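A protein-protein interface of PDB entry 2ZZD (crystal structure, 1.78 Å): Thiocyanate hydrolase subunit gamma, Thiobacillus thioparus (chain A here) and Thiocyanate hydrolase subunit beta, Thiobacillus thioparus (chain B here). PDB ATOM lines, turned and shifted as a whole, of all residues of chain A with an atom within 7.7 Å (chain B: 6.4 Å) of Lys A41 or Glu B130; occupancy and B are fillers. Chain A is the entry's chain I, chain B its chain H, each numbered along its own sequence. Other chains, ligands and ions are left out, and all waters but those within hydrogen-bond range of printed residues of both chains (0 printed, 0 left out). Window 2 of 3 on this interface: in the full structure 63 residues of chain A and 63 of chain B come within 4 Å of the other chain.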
ATOM      1  N   ALA A  33       6.002 -10.828  -6.846  1.00  0.00           N
ATOM      2  CA  ALA A  33       5.754  -9.987  -8.008  1.00  0.00           C
ATOM      3  C   ALA A  33       4.386 -10.289  -8.607  1.00  0.00           C
ATOM      4  O   ALA A  33       3.604  -9.380  -8.894  1.00  0.00           O
ATOM      5  CB  ALA A  33       6.843 -10.210  -9.056  1.00  0.00           C
ATOM      6  N   ARG A  35       1.762 -11.867  -7.179  1.00  0.00           N
ATOM      7  CA  ARG A  35       0.679 -11.542  -6.262  1.00  0.00           C
ATOM      8  C   ARG A  35       0.422 -10.038  -6.195  1.00  0.00           C
ATOM      9  O   ARG A  35      -0.730  -9.600  -6.245  1.00  0.00           O
ATOM     10  CB  ARG A  35       0.974 -12.094  -4.862  1.00  0.00           C
ATOM     11  CG  ARG A  35      -0.106 -11.781  -3.822  1.00  0.00           C
ATOM     12  CD  ARG A  35      -0.141 -12.841  -2.731  1.00  0.00           C
ATOM     13  NE  ARG A  35       1.194 -13.191  -2.250  1.00  0.00           N
ATOM     14  CZ  ARG A  35       1.809 -12.610  -1.225  1.00  0.00           C
ATOM     15  NH1 ARG A  35       1.215 -11.636  -0.548  1.00  0.00           N
ATOM     16  NH2 ARG A  35       3.023 -13.013  -0.877  1.00  0.00           N
ATOM     17  N   GLU A  36       1.478  -9.236  -6.094  1.00  0.00           N
ATOM     18  CA  GLU A  36       1.279  -7.795  -6.035  1.00  0.00           C
ATOM     19  C   GLU A  36       0.643  -7.269  -7.322  1.00  0.00           C
ATOM     20  O   GLU A  36      -0.265  -6.445  -7.270  1.00  0.00           O
ATOM     21  CB  GLU A  36       2.597  -7.066  -5.747  1.00  0.00           C
ATOM     22  CG  GLU A  36       3.051  -7.223  -4.292  1.00  0.00           C
ATOM     23  CD  GLU A  36       4.148  -6.251  -3.886  1.00  0.00           C
ATOM     24  OE1 GLU A  36       4.542  -6.271  -2.702  1.00  0.00           O
ATOM     25  OE2 GLU A  36       4.615  -5.466  -4.740  1.00  0.00           O
ATOM     26  N   LEU A  37       1.104  -7.751  -8.472  1.00  0.00           N
ATOM     27  CA  LEU A  37       0.544  -7.307  -9.745  1.00  0.00           C
ATOM     28  C   LEU A  37      -0.930  -7.683  -9.881  1.00  0.00           C
ATOM     29  O   LEU A  37      -1.740  -6.873 -10.333  1.00  0.00           O
ATOM     30  CB  LEU A  37       1.342  -7.896 -10.917  1.00  0.00           C
ATOM     31  CG  LEU A  37       2.719  -7.265 -11.143  1.00  0.00           C
ATOM     32  CD1 LEU A  37       3.538  -8.134 -12.091  1.00  0.00           C
ATOM     33  CD2 LEU A  37       2.553  -5.855 -11.706  1.00  0.00           C
ATOM     34  N   ALA A  38      -1.281  -8.905  -9.489  1.00  0.00           N
ATOM     35  CA  ALA A  38      -2.668  -9.355  -9.588  1.00  0.00           C
ATOM     36  C   ALA A  38      -3.585  -8.496  -8.718  1.00  0.00           C
ATOM     37  O   ALA A  38      -4.692  -8.139  -9.122  1.00  0.00           O
ATOM     38  CB  ALA A  38      -2.780 -10.821  -9.178  1.00  0.00           C
ATOM     39  N   ILE A  39      -3.123  -8.164  -7.519  1.00  0.00           N
ATOM     40  CA  ILE A  39      -3.929  -7.349  -6.622  1.00  0.00           C
ATOM     41  C   ILE A  39      -3.999  -5.910  -7.138  1.00  0.00           C
ATOM     42  O   ILE A  39      -5.059  -5.282  -7.106  1.00  0.00           O
ATOM     43  CB  ILE A  39      -3.363  -7.402  -5.181  1.00  0.00           C
ATOM     44  CG1 ILE A  39      -3.557  -8.818  -4.621  1.00  0.00           C
ATOM     45  CG2 ILE A  39      -4.067  -6.372  -4.291  1.00  0.00           C
ATOM     46  CD1 ILE A  39      -2.893  -9.074  -3.280  1.00  0.00           C
ATOM     47  N   GLU A  40      -2.875  -5.394  -7.628  1.00  0.00           N
ATOM     48  CA  GLU A  40      -2.837  -4.032  -8.165  1.00  0.00           C
ATOM     49  C   GLU A  40      -3.780  -3.873  -9.359  1.00  0.00           C
ATOM     50  O   GLU A  40      -4.397  -2.822  -9.538  1.00  0.00           O
ATOM     51  CB  GLU A  40      -1.410  -3.664  -8.594  1.00  0.00           C
ATOM     52  CG  GLU A  40      -0.463  -3.392  -7.426  1.00  0.00           C
ATOM     53  CD  GLU A  40       0.998  -3.337  -7.844  1.00  0.00           C
ATOM     54  OE1 GLU A  40       1.291  -3.481  -9.053  1.00  0.00           O
ATOM     55  OE2 GLU A  40       1.861  -3.171  -6.957  1.00  0.00           O
ATOM     56  N   LYS A  41      -3.889  -4.919 -10.175  1.00  0.00           N
ATOM     57  CA  LYS A  41      -4.752  -4.880 -11.354  1.00  0.00           C
ATOM     58  C   LYS A  41      -6.192  -5.277 -11.043  1.00  0.00           C
ATOM     59  O   LYS A  41      -7.039  -5.308 -11.935  1.00  0.00           O
ATOM     60  CB  LYS A  41      -4.184  -5.783 -12.452  1.00  0.00           C
ATOM     61  CG  LYS A  41      -2.827  -5.339 -12.983  1.00  0.00           C
ATOM     62  CD  LYS A  41      -2.886  -3.932 -13.574  1.00  0.00           C
ATOM     63  CE  LYS A  41      -1.559  -3.552 -14.226  1.00  0.00           C
ATOM     64  NZ  LYS A  41      -1.564  -2.154 -14.753  1.00  0.00           N
ATOM     65  N   GLY A  42      -6.462  -5.587  -9.780  1.00  0.00           N
ATOM     66  CA  GLY A  42      -7.806  -5.960  -9.372  1.00  0.00           C
ATOM     67  C   GLY A  42      -8.296  -7.322  -9.836  1.00  0.00           C
ATOM     68  O   GLY A  42      -9.502  -7.552  -9.903  1.00  0.00           O
ATOM     69  N   LEU A  43      -7.375  -8.231 -10.149  1.00  0.00           N
ATOM     70  CA  LEU A  43      -7.756  -9.567 -10.615  1.00  0.00           C
ATOM     71  C   LEU A  43      -8.371 -10.361  -9.457  1.00  0.00           C
ATOM     72  O   LEU A  43      -9.377 -11.056  -9.632  1.00  0.00           O
ATOM     73  CB  LEU A  43      -6.537 -10.265 -11.217  1.00  0.00           C
ATOM     74  CG  LEU A  43      -5.866  -9.414 -12.306  1.00  0.00           C
ATOM     75  CD1 LEU A  43      -4.773 -10.219 -12.975  1.00  0.00           C
ATOM     76  CD2 LEU A  43      -6.894  -8.956 -13.342  1.00  0.00           C
ATOM     77  N   PHE A  44      -7.748 -10.283  -8.285  1.00  0.00           N
ATOM     78  CA  PHE A  44      -8.302 -10.889  -7.079  1.00  0.00           C
ATOM     79  C   PHE A  44      -7.871  -9.961  -5.954  1.00  0.00           C
ATOM     80  O   PHE A  44      -6.950  -9.164  -6.132  1.00  0.00           O
ATOM     81  CB  PHE A  44      -7.862 -12.357  -6.867  1.00  0.00           C
ATOM     82  CG  PHE A  44      -6.385 -12.565  -6.676  1.00  0.00           C
ATOM     83  CD1 PHE A  44      -5.765 -12.262  -5.465  1.00  0.00           C
ATOM     84  CD2 PHE A  44      -5.629 -13.160  -7.684  1.00  0.00           C
ATOM     85  CE1 PHE A  44      -4.411 -12.557  -5.257  1.00  0.00           C
ATOM     86  CE2 PHE A  44      -4.277 -13.460  -7.492  1.00  0.00           C
ATOM     87  CZ  PHE A  44      -3.666 -13.163  -6.281  1.00  0.00           C
ATOM     88  N   PHE B 125      -3.370  -8.565 -18.870  1.00  0.00           N
ATOM     89  CA  PHE B 125      -3.802  -7.916 -17.639  1.00  0.00           C
ATOM     90  C   PHE B 125      -2.615  -7.078 -17.145  1.00  0.00           C
ATOM     91  O   PHE B 125      -2.790  -6.073 -16.453  1.00  0.00           O
ATOM     92  CB  PHE B 125      -4.251  -8.962 -16.615  1.00  0.00           C
ATOM     93  CG  PHE B 125      -5.570  -9.612 -16.967  1.00  0.00           C
ATOM     94  CD1 PHE B 125      -6.721  -8.837 -17.112  1.00  0.00           C
ATOM     95  CD2 PHE B 125      -5.659 -10.984 -17.183  1.00  0.00           C
ATOM     96  CE1 PHE B 125      -7.944  -9.416 -17.469  1.00  0.00           C
ATOM     97  CE2 PHE B 125      -6.880 -11.579 -17.541  1.00  0.00           C
ATOM     98  CZ  PHE B 125      -8.025 -10.788 -17.685  1.00  0.00           C
ATOM     99  N   VAL B 126      -1.408  -7.505 -17.512  1.00  0.00           N
ATOM    100  CA  VAL B 126      -0.180  -6.772 -17.209  1.00  0.00           C
ATOM    101  C   VAL B 126       0.678  -6.890 -18.466  1.00  0.00           C
ATOM    102  O   VAL B 126       0.573  -7.878 -19.200  1.00  0.00           O
ATOM    103  CB  VAL B 126       0.656  -7.368 -16.029  1.00  0.00           C
ATOM    104  CG1 VAL B 126      -0.217  -7.567 -14.804  1.00  0.00           C
ATOM    105  CG2 VAL B 126       1.327  -8.661 -16.454  1.00  0.00           C
ATOM    106  N   THR B 127       1.509  -5.888 -18.732  1.00  0.00           N
ATOM    107  CA  THR B 127       2.398  -5.954 -19.882  1.00  0.00           C
ATOM    108  C   THR B 127       3.628  -6.707 -19.391  1.00  0.00           C
ATOM    109  O   THR B 127       3.864  -6.798 -18.184  1.00  0.00           O
ATOM    110  CB  THR B 127       2.849  -4.559 -20.357  1.00  0.00           C
ATOM    111  OG1 THR B 127       3.546  -3.893 -19.298  1.00  0.00           O
ATOM    112  CG2 THR B 127       1.654  -3.728 -20.789  1.00  0.00           C
ATOM    113  N   LEU B 128       4.411  -7.256 -20.311  1.00  0.00           N
ATOM    114  CA  LEU B 128       5.608  -7.966 -19.897  1.00  0.00           C
ATOM    115  C   LEU B 128       6.525  -6.956 -19.218  1.00  0.00           C
ATOM    116  O   LEU B 128       7.274  -7.289 -18.300  1.00  0.00           O
ATOM    117  CB  LEU B 128       6.319  -8.590 -21.098  1.00  0.00           C
ATOM    118  CG  LEU B 128       7.554  -9.423 -20.731  1.00  0.00           C
ATOM    119  CD1 LEU B 128       7.159 -10.533 -19.761  1.00  0.00           C
ATOM    120  CD2 LEU B 128       8.170 -10.017 -21.989  1.00  0.00           C
ATOM    121  N   THR B 129       6.453  -5.712 -19.680  1.00  0.00           N
ATOM    122  CA  THR B 129       7.264  -4.642 -19.121  1.00  0.00           C
ATOM    123  C   THR B 129       6.931  -4.442 -17.640  1.00  0.00           C
ATOM    124  O   THR B 129       7.830  -4.267 -16.815  1.00  0.00           O
ATOM    125  CB  THR B 129       7.043  -3.327 -19.897  1.00  0.00           C
ATOM    126  OG1 THR B 129       7.455  -3.511 -21.258  1.00  0.00           O
ATOM    127  CG2 THR B 129       7.855  -2.191 -19.283  1.00  0.00           C
ATOM    128  N   GLU B 130       5.647  -4.479 -17.300  1.00  0.00           N
ATOM    129  CA  GLU B 130       5.246  -4.317 -15.907  1.00  0.00           C
ATOM    130  C   GLU B 130       5.772  -5.475 -15.057  1.00  0.00           C
ATOM    131  O   GLU B 130       6.166  -5.277 -13.907  1.00  0.00           O
ATOM    132  CB  GLU B 130       3.722  -4.227 -15.790  1.00  0.00           C
ATOM    133  CG  GLU B 130       3.163  -2.895 -16.277  1.00  0.00           C
ATOM    134  CD  GLU B 130       1.648  -2.844 -16.240  1.00  0.00           C
ATOM    135  OE1 GLU B 130       1.012  -3.760 -16.803  1.00  0.00           O
ATOM    136  OE2 GLU B 130       1.092  -1.888 -15.657  1.00  0.00           O
ATOM    137  N   LEU B 131       5.777  -6.681 -15.620  1.00  0.00           N
ATOM    138  CA  LEU B 131       6.278  -7.845 -14.893  1.00  0.00           C
ATOM    139  C   LEU B 131       7.791  -7.727 -14.696  1.00  0.00           C
ATOM    140  O   LEU B 131       8.297  -7.937 -13.592  1.00  0.00           O
ATOM    141  CB  LEU B 131       5.952  -9.142 -15.644  1.00  0.00           C
ATOM    142  CG  LEU B 131       6.501 -10.436 -15.024  1.00  0.00           C
ATOM    143  CD1 LEU B 131       5.977 -10.602 -13.600  1.00  0.00           C
ATOM    144  CD2 LEU B 131       6.083 -11.634 -15.875  1.00  0.00           C
ATOM    145  N   HIS B 132       8.514  -7.397 -15.764  1.00  0.00           N
ATOM    146  CA  HIS B 132       9.962  -7.241 -15.670  1.00  0.00           C
ATOM    147  C   HIS B 132      10.306  -6.156 -14.650  1.00  0.00           C
ATOM    148  O   HIS B 132      11.182  -6.343 -13.808  1.00  0.00           O
ATOM    149  CB  HIS B 132      10.565  -6.865 -17.030  1.00  0.00           C
ATOM    150  CG  HIS B 132      10.611  -7.998 -18.010  1.00  0.00           C
ATOM    151  ND1 HIS B 132      10.992  -7.830 -19.324  1.00  0.00           N
ATOM    152  CD2 HIS B 132      10.345  -9.318 -17.863  1.00  0.00           C
ATOM    153  CE1 HIS B 132      10.958  -8.996 -19.946  1.00  0.00           C
ATOM    154  NE2 HIS B 132      10.568  -9.916 -19.080  1.00  0.00           N
ATOM    155  N   ASN B 133       9.610  -5.024 -14.727  1.00  0.00           N
ATOM    156  CA  ASN B 133       9.854  -3.918 -13.805  1.00  0.00           C
ATOM    157  C   ASN B 133       9.562  -4.292 -12.352  1.00  0.00           C
ATOM    158  O   ASN B 133      10.292  -3.883 -11.442  1.00  0.00           O
ATOM    159  CB  ASN B 133       9.013  -2.698 -14.196  1.00  0.00           C
ATOM    160  CG  ASN B 133       9.514  -2.026 -15.461  1.00  0.00           C
ATOM    161  OD1 ASN B 133      10.585  -2.354 -15.969  1.00  0.00           O
ATOM    162  ND2 ASN B 133       8.742  -1.072 -15.968  1.00  0.00           N
ATOM    163  N   LYS B 134       8.495  -5.059 -12.129  1.00  0.00           N
ATOM    164  CA  LYS B 134       8.134  -5.472 -10.772  1.00  0.00           C
ATOM    165  C   LYS B 134       9.222  -6.383 -10.190  1.00  0.00           C
ATOM    166  O   LYS B 134       9.548  -6.297  -9.004  1.00  0.00           O
ATOM    167  CB  LYS B 134       6.766  -6.182 -10.773  1.00  0.00           C
ATOM    168  CG  LYS B 134       6.350  -6.790  -9.423  1.00  0.00           C
ATOM    169  CD  LYS B 134       6.096  -5.739  -8.335  1.00  0.00           C
ATOM    170  CE  LYS B 134       4.748  -5.034  -8.494  1.00  0.00           C
ATOM    171  NZ  LYS B 134       4.419  -4.185  -7.301  1.00  0.00           N
ATOM    172  N   ILE B 135       9.793  -7.245 -11.026  1.00  0.00           N
ATOM    173  CA  ILE B 135      10.849  -8.142 -10.570  1.00  0.00           C
ATOM    174  C   ILE B 135      12.087  -7.332 -10.197  1.00  0.00           C
ATOM    175  O   ILE B 135      12.725  -7.590  -9.173  1.00  0.00           O
ATOM    176  CB  ILE B 135      11.193  -9.188 -11.662  1.00  0.00           C
ATOM    177  CG1 ILE B 135      10.026 -10.175 -11.798  1.00  0.00           C
ATOM    178  CG2 ILE B 135      12.482  -9.929 -11.308  1.00  0.00           C
ATOM    179  CD1 ILE B 135      10.083 -11.051 -13.046  1.00  0.00           C
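NZ of Lys A41 lies within salt-bridge range of OE2 of Glu B130, 2.8 Å away.
The side-chain carboxylate of Glu A36 lies within salt-bridge range of the side-chain amino group of Lys B134.
The side-chain carboxylate (OE2) of Glu A40 is in salt-bridge range of the side-chain amino group (NZ) of Lys B134 (2.8 Å).
The backbone NH (N) of Thr B127 is in hydrogen-bond range of the side-chain carboxylate (OE1) of Glu B130, 2.9 Å away.
N of Leu A43 lies within hydrogen-bond range of O of Ala A38 (2.9 Å).
Lys B134 touches Ala A33 (CG to CB, 3.5 Å).
CD1 of Leu B131 touches CD1 of Leu A37 (3.8 Å).
Lys B134 touches Leu A37.
O of Phe B125 touches CG of Lys A41, 3.5 Å away.
Lys A41 touches Val B126.
CD1 of Phe B125 touches CD2 of Leu A43, 3.8 Å away.
Printed residues of chain B that touch a printed residue of chain A: Phe B125, Val B126, Glu B130, Leu B131 and Lys B134.
Hydrophobic or aromatic side chains of chain B that line the printed part of chain A: Phe B125, Val B126 and Leu B131.
Of the 11 printed residues of chain A, 6 touch a printed residue of chain B.
Printed residues of chain A that touch a printed residue of chain B: Ala A33, Glu A36, Leu A37, Glu A40, Lys A41 and Leu A43.
Hydrophobic or aromatic side chains of chain A that line the printed part of chain B: Ala A33, Leu A37 and Leu A43.
Of the printed residues of chain B, Lys A41 touches Phe B125 (3.5 Å), Val B126 (3.9 Å) and Glu B130 (2.8 Å).
Of chain A, only Lys A41 (2.8 Å) comes within 4 Å of Glu B130.
Of the printed residues of chain B, Glu A36 touches Lys B134 (2.9 Å).
Of the printed residues of chain A, Val B126 touches Lys A41 (3.9 Å).
Printed residues of chain B within 4 Å of Glu A40: Lys B134.
The nearest residue of chain B that does not touch Lys A41 is Thr B127 (5.9 Å).
The nearest residue of chain A that does not touch Glu B130 is Leu A37 (4.3 Å).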
